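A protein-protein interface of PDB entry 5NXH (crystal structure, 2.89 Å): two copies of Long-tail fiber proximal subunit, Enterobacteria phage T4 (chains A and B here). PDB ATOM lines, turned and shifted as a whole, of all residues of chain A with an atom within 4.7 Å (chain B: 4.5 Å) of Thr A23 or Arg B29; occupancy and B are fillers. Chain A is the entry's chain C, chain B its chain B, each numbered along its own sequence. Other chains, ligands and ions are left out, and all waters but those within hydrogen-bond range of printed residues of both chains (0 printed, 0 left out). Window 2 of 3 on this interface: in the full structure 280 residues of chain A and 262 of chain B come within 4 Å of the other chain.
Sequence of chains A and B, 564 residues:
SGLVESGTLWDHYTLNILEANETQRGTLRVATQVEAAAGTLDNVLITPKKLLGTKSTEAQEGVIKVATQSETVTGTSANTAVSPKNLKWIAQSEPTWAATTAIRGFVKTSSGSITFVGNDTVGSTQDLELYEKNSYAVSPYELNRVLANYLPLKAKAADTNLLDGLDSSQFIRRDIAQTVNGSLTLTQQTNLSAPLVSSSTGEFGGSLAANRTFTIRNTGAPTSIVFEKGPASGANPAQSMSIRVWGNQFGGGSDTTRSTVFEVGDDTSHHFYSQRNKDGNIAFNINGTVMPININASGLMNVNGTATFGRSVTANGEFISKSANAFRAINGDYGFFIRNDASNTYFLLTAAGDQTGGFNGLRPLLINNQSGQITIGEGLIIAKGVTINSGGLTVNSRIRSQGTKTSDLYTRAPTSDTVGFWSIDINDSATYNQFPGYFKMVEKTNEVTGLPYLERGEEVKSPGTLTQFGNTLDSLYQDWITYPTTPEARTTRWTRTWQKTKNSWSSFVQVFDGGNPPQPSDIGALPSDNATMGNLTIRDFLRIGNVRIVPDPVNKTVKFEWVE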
ATOM      1  N   ASN A  21      24.882 -19.382  12.310  1.00  0.00           N
ATOM      2  CA  ASN A  21      24.368 -19.802  11.003  1.00  0.00           C
ATOM      3  C   ASN A  21      25.363 -19.421   9.858  1.00  0.00           C
ATOM      4  O   ASN A  21      26.589 -19.292  10.087  1.00  0.00           O
ATOM      5  CB  ASN A  21      22.890 -19.351  10.821  1.00  0.00           C
ATOM      6  CG  ASN A  21      22.724 -17.841  10.667  1.00  0.00           C
ATOM      7  OD1 ASN A  21      23.604 -17.070  11.031  1.00  0.00           O
ATOM      8  ND2 ASN A  21      21.617 -17.414  10.081  1.00  0.00           N
ATOM      9  N   GLU A  22      24.854 -19.340   8.632  1.00  0.00           N
ATOM     10  CA  GLU A  22      25.694 -19.070   7.463  1.00  0.00           C
ATOM     11  C   GLU A  22      25.885 -17.575   7.186  1.00  0.00           C
ATOM     12  O   GLU A  22      26.704 -17.181   6.377  1.00  0.00           O
ATOM     13  CB  GLU A  22      25.175 -19.836   6.233  1.00  0.00           C
ATOM     14  CG  GLU A  22      23.716 -19.643   5.865  1.00  0.00           C
ATOM     15  CD  GLU A  22      23.123 -20.861   5.165  1.00  0.00           C
ATOM     16  OE1 GLU A  22      23.885 -21.664   4.569  1.00  0.00           O
ATOM     17  OE2 GLU A  22      21.893 -21.009   5.233  1.00  0.00           O
ATOM     18  N   THR A  23      25.092 -16.745   7.844  1.00  0.00           N
ATOM     19  CA  THR A  23      25.215 -15.281   7.856  1.00  0.00           C
ATOM     20  C   THR A  23      26.128 -14.829   9.010  1.00  0.00           C
ATOM     21  O   THR A  23      27.264 -14.439   8.778  1.00  0.00           O
ATOM     22  CB  THR A  23      23.811 -14.617   7.970  1.00  0.00           C
ATOM     23  OG1 THR A  23      23.061 -15.162   9.077  1.00  0.00           O
ATOM     24  CG2 THR A  23      22.990 -14.806   6.689  1.00  0.00           C
ATOM     25  N   GLN A  24      25.661 -14.941  10.260  1.00  0.00           N
ATOM     26  CA  GLN A  24      26.449 -14.577  11.471  1.00  0.00           C
ATOM     27  C   GLN A  24      27.319 -15.740  11.998  1.00  0.00           C
ATOM     28  O   GLN A  24      26.988 -16.913  11.811  1.00  0.00           O
ATOM     29  CB  GLN A  24      25.515 -14.069  12.581  1.00  0.00           C
ATOM     30  CG  GLN A  24      26.157 -13.511  13.859  1.00  0.00           C
ATOM     31  CD  GLN A  24      27.053 -12.296  13.647  1.00  0.00           C
ATOM     32  OE1 GLN A  24      28.224 -12.294  14.039  1.00  0.00           O
ATOM     33  NE2 GLN A  24      26.501 -11.250  13.048  1.00  0.00           N
ATOM     34  N   ARG A  25      28.422 -15.386  12.667  1.00  0.00           N
ATOM     35  CA  ARG A  25      29.279 -16.345  13.394  1.00  0.00           C
ATOM     36  C   ARG A  25      28.614 -16.819  14.688  1.00  0.00           C
ATOM     37  O   ARG A  25      27.647 -16.216  15.141  1.00  0.00           O
ATOM     38  CB  ARG A  25      30.624 -15.717  13.739  1.00  0.00           C
ATOM     39  CG  ARG A  25      31.501 -15.450  12.534  1.00  0.00           C
ATOM     40  CD  ARG A  25      32.713 -14.641  12.944  1.00  0.00           C
ATOM     41  NE  ARG A  25      33.496 -15.311  13.975  1.00  0.00           N
ATOM     42  CZ  ARG A  25      34.562 -14.793  14.584  1.00  0.00           C
ATOM     43  NH1 ARG A  25      35.018 -13.581  14.280  1.00  0.00           N
ATOM     44  NH2 ARG A  25      35.196 -15.502  15.509  1.00  0.00           N
ATOM     45  N   GLY A  26      29.136 -17.887  15.288  1.00  0.00           N
ATOM     46  CA  GLY A  26      28.548 -18.403  16.519  1.00  0.00           C
ATOM     47  C   GLY A  26      28.995 -19.739  17.094  1.00  0.00           C
ATOM     48  O   GLY A  26      29.910 -20.423  16.589  1.00  0.00           O
ATOM     49  N   LEU B  28      32.519 -19.631  14.867  1.00  0.00           N
ATOM     50  CA  LEU B  28      32.571 -19.570  13.399  1.00  0.00           C
ATOM     51  C   LEU B  28      31.190 -19.562  12.694  1.00  0.00           C
ATOM     52  O   LEU B  28      30.189 -20.035  13.224  1.00  0.00           O
ATOM     53  CB  LEU B  28      33.413 -20.745  12.880  1.00  0.00           C
ATOM     54  CG  LEU B  28      34.944 -20.674  13.026  1.00  0.00           C
ATOM     55  CD1 LEU B  28      35.534 -22.076  13.154  1.00  0.00           C
ATOM     56  CD2 LEU B  28      35.607 -19.887  11.886  1.00  0.00           C
ATOM     57  N   ARG B  29      31.177 -18.997  11.482  1.00  0.00           N
ATOM     58  CA  ARG B  29      30.028 -19.009  10.572  1.00  0.00           C
ATOM     59  C   ARG B  29      29.888 -20.395   9.940  1.00  0.00           C
ATOM     60  O   ARG B  29      30.897 -20.999   9.555  1.00  0.00           O
ATOM     61  CB  ARG B  29      30.294 -17.968   9.496  1.00  0.00           C
ATOM     62  CG  ARG B  29      29.341 -17.901   8.333  1.00  0.00           C
ATOM     63  CD  ARG B  29      29.904 -16.922   7.271  1.00  0.00           C
ATOM     64  NE  ARG B  29      30.716 -17.532   6.202  1.00  0.00           N
ATOM     65  CZ  ARG B  29      31.975 -17.202   5.873  1.00  0.00           C
ATOM     66  NH1 ARG B  29      32.636 -16.251   6.532  1.00  0.00           N
ATOM     67  NH2 ARG B  29      32.577 -17.848   4.878  1.00  0.00           N
ATOM     68  N   VAL B  30      28.661 -20.905   9.824  1.00  0.00           N
ATOM     69  CA  VAL B  30      28.426 -22.198   9.127  1.00  0.00           C
ATOM     70  C   VAL B  30      28.599 -22.033   7.613  1.00  0.00           C
ATOM     71  O   VAL B  30      28.204 -21.016   7.066  1.00  0.00           O
ATOM     72  CB  VAL B  30      27.075 -22.883   9.505  1.00  0.00           C
ATOM     73  CG1 VAL B  30      25.912 -22.565   8.559  1.00  0.00           C
ATOM     74  CG2 VAL B  30      27.247 -24.397   9.544  1.00  0.00           C
ATOM     75  N   ALA B  31      29.177 -23.036   6.955  1.00  0.00           N
ATOM     76  CA  ALA B  31      29.486 -22.962   5.520  1.00  0.00           C
ATOM     77  C   ALA B  31      28.253 -23.083   4.658  1.00  0.00           C
ATOM     78  O   ALA B  31      27.241 -23.654   5.071  1.00  0.00           O
ATOM     79  CB  ALA B  31      30.497 -24.034   5.120  1.00  0.00           C
ATOM     80  N   GLU B  35      30.839 -23.825  -0.725  1.00  0.00           N
ATOM     81  CA  GLU B  35      32.114 -23.657   0.002  1.00  0.00           C
ATOM     82  C   GLU B  35      32.624 -24.955   0.610  1.00  0.00           C
ATOM     83  O   GLU B  35      33.839 -25.197   0.637  1.00  0.00           O
ATOM     84  CB  GLU B  35      31.967 -22.670   1.156  1.00  0.00           C
ATOM     85  CG  GLU B  35      31.924 -21.195   0.809  1.00  0.00           C
ATOM     86  CD  GLU B  35      31.662 -20.344   2.060  1.00  0.00           C
ATOM     87  OE1 GLU B  35      30.846 -20.747   2.907  1.00  0.00           O
ATOM     88  OE2 GLU B  35      32.337 -19.286   2.269  1.00  0.00           O
ATOM     89  N   VAL B  44      35.601 -21.761   8.172  1.00  0.00           N
ATOM     90  CA  VAL B  44      34.141 -21.981   8.079  1.00  0.00           C
ATOM     91  C   VAL B  44      33.769 -23.367   8.626  1.00  0.00           C
ATOM     92  O   VAL B  44      34.586 -24.279   8.578  1.00  0.00           O
ATOM     93  CB  VAL B  44      33.602 -21.841   6.619  1.00  0.00           C
ATOM     94  CG1 VAL B  44      32.161 -21.420   6.653  1.00  0.00           C
ATOM     95  CG2 VAL B  44      34.389 -20.814   5.805  1.00  0.00           C
ATOM     96  N   LEU B  45      32.542 -23.526   9.135  1.00  0.00           N
ATOM     97  CA  LEU B  45      32.090 -24.782   9.774  1.00  0.00           C
ATOM     98  C   LEU B  45      31.418 -25.789   8.830  1.00  0.00           C
ATOM     99  O   LEU B  45      30.903 -25.403   7.794  1.00  0.00           O
ATOM    100  CB  LEU B  45      31.114 -24.455  10.915  1.00  0.00           C
ATOM    101  CG  LEU B  45      31.598 -23.692  12.140  1.00  0.00           C
ATOM    102  CD1 LEU B  45      30.498 -23.684  13.197  1.00  0.00           C
ATOM    103  CD2 LEU B  45      32.887 -24.266  12.729  1.00  0.00           C
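N of Gly A26 sits at hydrogen-bond distance from O of Leu B28, 3.2 Å away.
The backbone carbonyl oxygen (O) of Asn A21 sits at hydrogen-bond distance from the backbone NH (N) of Val B30 (2.6 Å).
The guanidinium group (NH2) of Arg B29 lies within salt-bridge range of the side-chain carboxylate (OE2) of Glu B35 (3.0 Å).
N of Leu B45 is in hydrogen-bond range of O of Arg B29.
N of Ala B31 sits close to O of Leu B45 (3.0 Å).
The side-chain hydroxyl (OG1) of Thr A23 sits at hydrogen-bond distance from the side-chain amide oxygen (OD1) of Asn A21.
The side-chain amide oxygen (OD1) of Asn A21 is in hydrogen-bond range of the backbone NH (N) of Gln A24, at 3.1 Å.
Arg B29 touches Asn A21.
Arg B29 touches Glu A22.
O of Val B30 touches CA of Glu A22, 3.2 Å away.
Glu A22 touches Ala B31.
Arg B29 touches Thr A23.
Arg B29 touches Gln A24 (CA to O, 3.9 Å).
O of Leu B28 touches CA of Arg A25, at 3.8 Å.
Arg B29 touches Arg A25.
Of the printed residues of chain B, Thr A23 touches Arg B29.
Printed residues of chain B within 4 Å of Gln A24: Arg B29.
Of the printed residues of chain B, Arg A25 touches Leu B28 and Arg B29.
Of the printed residues of chain B, Gly A26 touches Leu B28 (3.2 Å).
Of the printed residues of chain A, Leu B28 touches Arg A25 and Gly A26.
Leu B45 touches none of the printed residues of chain A.
The nearest printed residue of chain B that does not touch Thr A23 is Val B30 (5.3 Å).
The nearest residue of chain A that does not touch Arg B29 is Gly A26 (4.5 Å).
The nearest printed residue of chain B that does not touch Asn A21 is Leu B28 (4.8 Å).
Hydrophobic or aromatic side chains of chain B that line the printed part of chain A: Val B30.
Of the 6 printed residues of chain A, 6 touch a printed residue of chain B.
Among the printed residues, 10 pairs touch across the chains.
No position is printed for both chains.
Of the 10 pairs that touch across the chains among the printed residues, none has its exchanged pair printed and touching as well.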
